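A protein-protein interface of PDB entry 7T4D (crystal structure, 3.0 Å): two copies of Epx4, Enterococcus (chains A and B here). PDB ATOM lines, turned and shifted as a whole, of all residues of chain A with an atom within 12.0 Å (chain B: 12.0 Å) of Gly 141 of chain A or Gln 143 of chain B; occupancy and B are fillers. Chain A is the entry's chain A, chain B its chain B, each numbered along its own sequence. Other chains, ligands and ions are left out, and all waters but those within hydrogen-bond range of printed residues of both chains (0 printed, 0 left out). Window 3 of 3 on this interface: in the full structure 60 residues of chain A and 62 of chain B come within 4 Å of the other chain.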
ATOM      1  N   ILE A 137      26.752 -32.137 -10.928  1.00  0.00           N
ATOM      2  CA  ILE A 137      27.870 -31.286 -10.556  1.00  0.00           C
ATOM      3  C   ILE A 137      27.426 -30.380  -9.419  1.00  0.00           C
ATOM      4  O   ILE A 137      26.229 -30.207  -9.184  1.00  0.00           O
ATOM      5  CB  ILE A 137      28.368 -30.439 -11.740  1.00  0.00           C
ATOM      6  CG1 ILE A 137      27.214 -29.637 -12.345  1.00  0.00           C
ATOM      7  CG2 ILE A 137      29.013 -31.324 -12.796  1.00  0.00           C
ATOM      8  CD1 ILE A 137      27.579 -28.915 -13.620  1.00  0.00           C
ATOM      9  N   LYS A 138      28.385 -29.799  -8.711  1.00  0.00           N
ATOM     10  CA  LYS A 138      28.061 -29.016  -7.532  1.00  0.00           C
ATOM     11  C   LYS A 138      29.018 -27.845  -7.370  1.00  0.00           C
ATOM     12  O   LYS A 138      30.117 -27.844  -7.926  1.00  0.00           O
ATOM     13  CB  LYS A 138      28.107 -29.905  -6.287  1.00  0.00           C
ATOM     14  CG  LYS A 138      27.354 -29.364  -5.086  1.00  0.00           C
ATOM     15  CD  LYS A 138      27.998 -29.828  -3.787  1.00  0.00           C
ATOM     16  CE  LYS A 138      28.416 -31.289  -3.857  1.00  0.00           C
ATOM     17  NZ  LYS A 138      29.138 -31.718  -2.625  1.00  0.00           N
ATOM     18  N   MET A 139      28.589 -26.845  -6.610  1.00  0.00           N
ATOM     19  CA  MET A 139      29.454 -25.729  -6.266  1.00  0.00           C
ATOM     20  C   MET A 139      29.168 -25.278  -4.840  1.00  0.00           C
ATOM     21  O   MET A 139      28.119 -24.697  -4.562  1.00  0.00           O
ATOM     22  CB  MET A 139      29.266 -24.570  -7.247  1.00  0.00           C
ATOM     23  CG  MET A 139      30.229 -24.592  -8.427  1.00  0.00           C
ATOM     24  SD  MET A 139      31.907 -24.093  -7.993  1.00  0.00           S
ATOM     25  CE  MET A 139      31.717 -22.316  -7.879  1.00  0.00           C
ATOM     26  N   GLU A 140      30.110 -25.545  -3.944  1.00  0.00           N
ATOM     27  CA  GLU A 140      30.005 -25.091  -2.566  1.00  0.00           C
ATOM     28  C   GLU A 140      30.941 -23.906  -2.382  1.00  0.00           C
ATOM     29  O   GLU A 140      32.147 -24.077  -2.204  1.00  0.00           O
ATOM     30  CB  GLU A 140      30.353 -26.217  -1.590  1.00  0.00           C
ATOM     31  CG  GLU A 140      29.307 -27.323  -1.499  1.00  0.00           C
ATOM     32  CD  GLU A 140      28.099 -26.926  -0.669  1.00  0.00           C
ATOM     33  OE1 GLU A 140      28.100 -25.807  -0.112  1.00  0.00           O
ATOM     34  OE2 GLU A 140      27.151 -27.735  -0.569  1.00  0.00           O
ATOM     35  N   GLY A 141      30.382 -22.703  -2.426  1.00  0.00           N
ATOM     36  CA  GLY A 141      31.191 -21.500  -2.411  1.00  0.00           C
ATOM     37  C   GLY A 141      31.950 -21.368  -3.717  1.00  0.00           C
ATOM     38  O   GLY A 141      31.365 -21.055  -4.754  1.00  0.00           O
ATOM     39  N   LYS A 142      33.257 -21.605  -3.669  1.00  0.00           N
ATOM     40  CA  LYS A 142      34.085 -21.587  -4.872  1.00  0.00           C
ATOM     41  C   LYS A 142      34.723 -22.948  -5.125  1.00  0.00           C
ATOM     42  O   LYS A 142      35.627 -23.076  -5.953  1.00  0.00           O
ATOM     43  CB  LYS A 142      35.169 -20.514  -4.765  1.00  0.00           C
ATOM     44  CG  LYS A 142      34.752 -19.150  -5.291  1.00  0.00           C
ATOM     45  CD  LYS A 142      35.889 -18.147  -5.175  1.00  0.00           C
ATOM     46  CE  LYS A 142      35.399 -16.808  -4.656  1.00  0.00           C
ATOM     47  NZ  LYS A 142      36.423 -15.742  -4.836  1.00  0.00           N
ATOM     48  N   GLN A 143      34.248 -23.965  -4.412  1.00  0.00           N
ATOM     49  CA  GLN A 143      34.799 -25.308  -4.543  1.00  0.00           C
ATOM     50  C   GLN A 143      33.856 -26.221  -5.317  1.00  0.00           C
ATOM     51  O   GLN A 143      32.735 -26.483  -4.879  1.00  0.00           O
ATOM     52  CB  GLN A 143      35.090 -25.909  -3.168  1.00  0.00           C
ATOM     53  CG  GLN A 143      35.308 -27.414  -3.194  1.00  0.00           C
ATOM     54  CD  GLN A 143      35.799 -27.958  -1.868  1.00  0.00           C
ATOM     55  OE1 GLN A 143      35.105 -28.731  -1.207  1.00  0.00           O
ATOM     56  NE2 GLN A 143      37.004 -27.561  -1.473  1.00  0.00           N
ATOM     57  N   PRO A 144      34.316 -26.713  -6.476  1.00  0.00           N
ATOM     58  CA  PRO A 144      33.488 -27.559  -7.337  1.00  0.00           C
ATOM     59  C   PRO A 144      33.288 -28.949  -6.751  1.00  0.00           C
ATOM     60  O   PRO A 144      33.959 -29.330  -5.791  1.00  0.00           O
ATOM     61  CB  PRO A 144      34.292 -27.625  -8.636  1.00  0.00           C
ATOM     62  CG  PRO A 144      35.703 -27.463  -8.198  1.00  0.00           C
ATOM     63  CD  PRO A 144      35.660 -26.501  -7.040  1.00  0.00           C
ATOM     64  N   GLY A 145      32.363 -29.696  -7.338  1.00  0.00           N
ATOM     65  CA  GLY A 145      32.090 -31.055  -6.921  1.00  0.00           C
ATOM     66  C   GLY A 145      31.433 -31.807  -8.055  1.00  0.00           C
ATOM     67  O   GLY A 145      30.880 -31.202  -8.974  1.00  0.00           O
ATOM     68  N   ALA A 146      31.485 -33.131  -7.990  1.00  0.00           N
ATOM     69  CA  ALA A 146      30.884 -33.967  -9.018  1.00  0.00           C
ATOM     70  C   ALA A 146      30.429 -35.273  -8.394  1.00  0.00           C
ATOM     71  O   ALA A 146      30.863 -35.631  -7.299  1.00  0.00           O
ATOM     72  CB  ALA A 146      31.864 -34.223 -10.150  1.00  0.00           C
ATOM     73  N   GLY B 136      19.419 -26.430  -8.429  1.00  0.00           N
ATOM     74  CA  GLY B 136      19.020 -25.538  -7.361  1.00  0.00           C
ATOM     75  C   GLY B 136      20.149 -24.679  -6.836  1.00  0.00           C
ATOM     76  O   GLY B 136      21.319 -24.909  -7.140  1.00  0.00           O
ATOM     77  N   ILE B 137      19.788 -23.682  -6.038  1.00  0.00           N
ATOM     78  CA  ILE B 137      20.761 -22.815  -5.393  1.00  0.00           C
ATOM     79  C   ILE B 137      20.518 -22.821  -3.886  1.00  0.00           C
ATOM     80  O   ILE B 137      19.440 -23.200  -3.427  1.00  0.00           O
ATOM     81  CB  ILE B 137      20.691 -21.379  -5.935  1.00  0.00           C
ATOM     82  CG1 ILE B 137      19.263 -20.840  -5.841  1.00  0.00           C
ATOM     83  CG2 ILE B 137      21.168 -21.334  -7.377  1.00  0.00           C
ATOM     84  CD1 ILE B 137      19.072 -19.499  -6.513  1.00  0.00           C
ATOM     85  N   LYS B 138      21.518 -22.400  -3.122  1.00  0.00           N
ATOM     86  CA  LYS B 138      21.442 -22.460  -1.668  1.00  0.00           C
ATOM     87  C   LYS B 138      22.201 -21.305  -1.033  1.00  0.00           C
ATOM     88  O   LYS B 138      23.024 -20.658  -1.682  1.00  0.00           O
ATOM     89  CB  LYS B 138      21.988 -23.793  -1.153  1.00  0.00           C
ATOM     90  CG  LYS B 138      23.474 -23.988  -1.406  1.00  0.00           C
ATOM     91  CD  LYS B 138      23.898 -25.437  -1.206  1.00  0.00           C
ATOM     92  CE  LYS B 138      24.455 -25.686   0.188  1.00  0.00           C
ATOM     93  NZ  LYS B 138      24.948 -27.086   0.335  1.00  0.00           N
ATOM     94  N   MET B 139      21.915 -21.047   0.238  1.00  0.00           N
ATOM     95  CA  MET B 139      22.648 -20.050   1.002  1.00  0.00           C
ATOM     96  C   MET B 139      22.880 -20.540   2.423  1.00  0.00           C
ATOM     97  O   MET B 139      21.945 -20.647   3.216  1.00  0.00           O
ATOM     98  CB  MET B 139      21.900 -18.715   1.020  1.00  0.00           C
ATOM     99  CG  MET B 139      22.318 -17.751  -0.079  1.00  0.00           C
ATOM    100  SD  MET B 139      23.921 -16.989   0.241  1.00  0.00           S
ATOM    101  CE  MET B 139      23.476 -15.780   1.488  1.00  0.00           C
ATOM    102  N   GLU B 140      24.137 -20.837   2.732  1.00  0.00           N
ATOM    103  CA  GLU B 140      24.524 -21.243   4.074  1.00  0.00           C
ATOM    104  C   GLU B 140      25.210 -20.077   4.768  1.00  0.00           C
ATOM    105  O   GLU B 140      26.391 -19.813   4.540  1.00  0.00           O
ATOM    106  CB  GLU B 140      25.452 -22.458   4.031  1.00  0.00           C
ATOM    107  CG  GLU B 140      24.769 -23.755   3.633  1.00  0.00           C
ATOM    108  CD  GLU B 140      25.724 -24.934   3.620  1.00  0.00           C
ATOM    109  OE1 GLU B 140      26.931 -24.726   3.864  1.00  0.00           O
ATOM    110  OE2 GLU B 140      25.267 -26.069   3.367  1.00  0.00           O
ATOM    111  N   GLY B 141      24.464 -19.377   5.616  1.00  0.00           N
ATOM    112  CA  GLY B 141      24.965 -18.164   6.228  1.00  0.00           C
ATOM    113  C   GLY B 141      25.087 -17.088   5.168  1.00  0.00           C
ATOM    114  O   GLY B 141      24.085 -16.541   4.708  1.00  0.00           O
ATOM    115  N   LYS B 142      26.321 -16.781   4.782  1.00  0.00           N
ATOM    116  CA  LYS B 142      26.567 -15.823   3.711  1.00  0.00           C
ATOM    117  C   LYS B 142      27.299 -16.479   2.541  1.00  0.00           C
ATOM    118  O   LYS B 142      27.792 -15.792   1.646  1.00  0.00           O
ATOM    119  CB  LYS B 142      27.367 -14.627   4.235  1.00  0.00           C
ATOM    120  CG  LYS B 142      26.501 -13.493   4.766  1.00  0.00           C
ATOM    121  CD  LYS B 142      27.344 -12.324   5.250  1.00  0.00           C
ATOM    122  CE  LYS B 142      26.830 -11.777   6.574  1.00  0.00           C
ATOM    123  NZ  LYS B 142      27.432 -10.454   6.898  1.00  0.00           N
ATOM    124  N   GLN B 143      27.362 -17.809   2.551  1.00  0.00           N
ATOM    125  CA  GLN B 143      28.057 -18.557   1.506  1.00  0.00           C
ATOM    126  C   GLN B 143      27.089 -19.261   0.557  1.00  0.00           C
ATOM    127  O   GLN B 143      26.321 -20.127   0.975  1.00  0.00           O
ATOM    128  CB  GLN B 143      29.007 -19.587   2.118  1.00  0.00           C
ATOM    129  CG  GLN B 143      29.477 -20.639   1.127  1.00  0.00           C
ATOM    130  CD  GLN B 143      30.570 -21.528   1.684  1.00  0.00           C
ATOM    131  OE1 GLN B 143      31.234 -21.177   2.660  1.00  0.00           O
ATOM    132  NE2 GLN B 143      30.761 -22.688   1.067  1.00  0.00           N
ATOM    133  N   PRO B 144      27.127 -18.885  -0.730  1.00  0.00           N
ATOM    134  CA  PRO B 144      26.231 -19.428  -1.756  1.00  0.00           C
ATOM    135  C   PRO B 144      26.557 -20.871  -2.132  1.00  0.00           C
ATOM    136  O   PRO B 144      27.607 -21.393  -1.759  1.00  0.00           O
ATOM    137  CB  PRO B 144      26.464 -18.502  -2.959  1.00  0.00           C
ATOM    138  CG  PRO B 144      27.167 -17.299  -2.410  1.00  0.00           C
ATOM    139  CD  PRO B 144      27.972 -17.803  -1.258  1.00  0.00           C
ATOM    140  N   GLY B 145      25.649 -21.501  -2.871  1.00  0.00           N
ATOM    141  CA  GLY B 145      25.852 -22.851  -3.359  1.00  0.00           C
ATOM    142  C   GLY B 145      24.971 -23.125  -4.561  1.00  0.00           C
ATOM    143  O   GLY B 145      23.958 -22.454  -4.765  1.00  0.00           O
ATOM    144  N   ALA B 146      25.350 -24.119  -5.357  1.00  0.00           N
ATOM    145  CA  ALA B 146      24.574 -24.483  -6.535  1.00  0.00           C
ATOM    146  C   ALA B 146      24.756 -25.957  -6.863  1.00  0.00           C
ATOM    147  O   ALA B 146      25.692 -26.600  -6.385  1.00  0.00           O
ATOM    148  CB  ALA B 146      24.971 -23.625  -7.723  1.00  0.00           C
ATOM    149  N   ASN B 147      23.854 -26.486  -7.678  1.00  0.00           N
ATOM    150  CA  ASN B 147      23.873 -27.897  -8.030  1.00  0.00           C
ATOM    151  C   ASN B 147      23.050 -28.166  -9.281  1.00  0.00           C
ATOM    152  O   ASN B 147      21.964 -27.613  -9.449  1.00  0.00           O
ATOM    153  CB  ASN B 147      23.363 -28.752  -6.867  1.00  0.00           C
ATOM    154  CG  ASN B 147      21.951 -28.395  -6.455  1.00  0.00           C
ATOM    155  OD1 ASN B 147      20.980 -28.940  -6.983  1.00  0.00           O
ATOM    156  ND2 ASN B 147      21.827 -27.477  -5.501  1.00  0.00           N
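NZ of Lys 138 of chain B lies within salt-bridge range of OE2 of Glu 140 of chain A. The backbone carbonyl oxygen (O) of Pro 144 of chain B is in hydrogen-bond range of the backbone NH (N) of Gly 141 of chain A, 3.1 Å away. The backbone NH (N) of Met 139 of chain A lies within hydrogen-bond range of the backbone carbonyl oxygen (O) of Ala 146 of chain B (2.9 Å).
The backbone carbonyl oxygen (O) of Asn 147 of chain B lies within hydrogen-bond range of the backbone NH (N) of Gly 136 of chain B (3.0 Å). The side-chain amino group (NZ) of Lys 138 of chain B is in salt-bridge range of the side-chain carboxylate (OE2) of Glu 140 of chain B (3.2 Å). The backbone NH of Lys 138 of chain B is in hydrogen-bond range of the backbone carbonyl oxygen of Gly 145 of chain B, 2.9 Å away. The backbone carbonyl oxygen (O) of Gly 145 of chain A lies within hydrogen-bond range of the backbone NH (N) of Lys 138 of chain A, at 2.9 Å.
Of the 10 printed residues of chain A, 5 touch a printed residue of chain B. Printed residues of chain A that touch a printed residue of chain B: Ile 137, Lys 138, Met 139, Glu 140 and Gly 141. Along chain A the printed residues that touch a printed residue of chain B span positions 137 to 141. Among the printed residues, 8 pairs touch across the chains. Among the printed residues, Asp or Glu carboxylates within 4 Å of a Lys or Arg side-chain nitrogen of the other chain: Glu 140 of chain A with Lys 138 of chain B (2.5 Å).
Glu 140 of chain A touches Lys 138 of chain B, but with the chains exchanged Lys 138 of chain A does not touch Glu 140 of chain B (8.5 Å). Glu 140 of chain A touches Gln 143 of chain B, but with the chains exchanged Gln 143 of chain A does not touch Glu 140 of chain B (10.4 Å). Gly 141 of chain A touches Gln 143 of chain B, but with the chains exchanged Gln 143 of chain A does not touch Gly 141 of chain B (14.7 Å). Gly 141 of chain A touches Pro 144 of chain B, but with the chains exchanged Pro 144 of chain A does not touch Gly 141 of chain B (17.2 Å). 10 positions are printed for both chains. Of the 8 pairs that touch across the chains among the printed residues, none has its exchanged pair printed and touching as well.
Of the printed residues of chain A, Gln 143 of chain B touches Glu 140 and Gly 141. Met 139 of chain A touches two residues of chain B. Of chain B, only Lys 138 (2.5 Å) and Gln 143 (3.7 Å) come within 4 Å of Glu 140 of chain A. No residue of chain B comes within 4 Å of Lys 142 of chain A. Of chain A, only Glu 140 comes within 4 Å of Lys 138 of chain B. Met 139 of chain B touches none of the printed residues of chain A. No residue of chain A comes within 4 Å of Glu 140 of chain B. No residue of chain A comes within 4 Å of Gly 141 of chain B. Of chain A, only Gly 141 comes within 4 Å of Pro 144 of chain B. Of chain A, only Met 139 (3.2 Å) comes within 4 Å of Gly 145 of chain B. Of the printed residues of chain A, Asn 147 of chain B touches Ile 137 (3.5 Å). Of the printed residues of chain B, Ile 137 of chain A touches Asn 147 (3.5 Å). Printed residues of chain B within 4 Å of Lys 138 of chain A: Ala 146 (3.5 Å). Ile 137 of chain B touches none of the printed residues of chain A. Gly 145 of chain A touches none of the printed residues of chain B. The nearest residue of chain A that does not touch Gln 143 of chain B is Lys 142 of chain A (5.5 Å). The nearest printed residue of chain A that does not touch Asn 147 of chain B is Lys 138 of chain A (4.4 Å).
Among the printed residues, pairs that only touch across the chains: Met 139 of chain A with Gly 145 of chain B, Lys 138 of chain A with Ala 146 of chain B, Ile 137 of chain A with Asn 147 of chain B, Gly 141 of chain A with Gln 143 of chain B and Glu 140 of chain A with Gln 143 of chain B.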
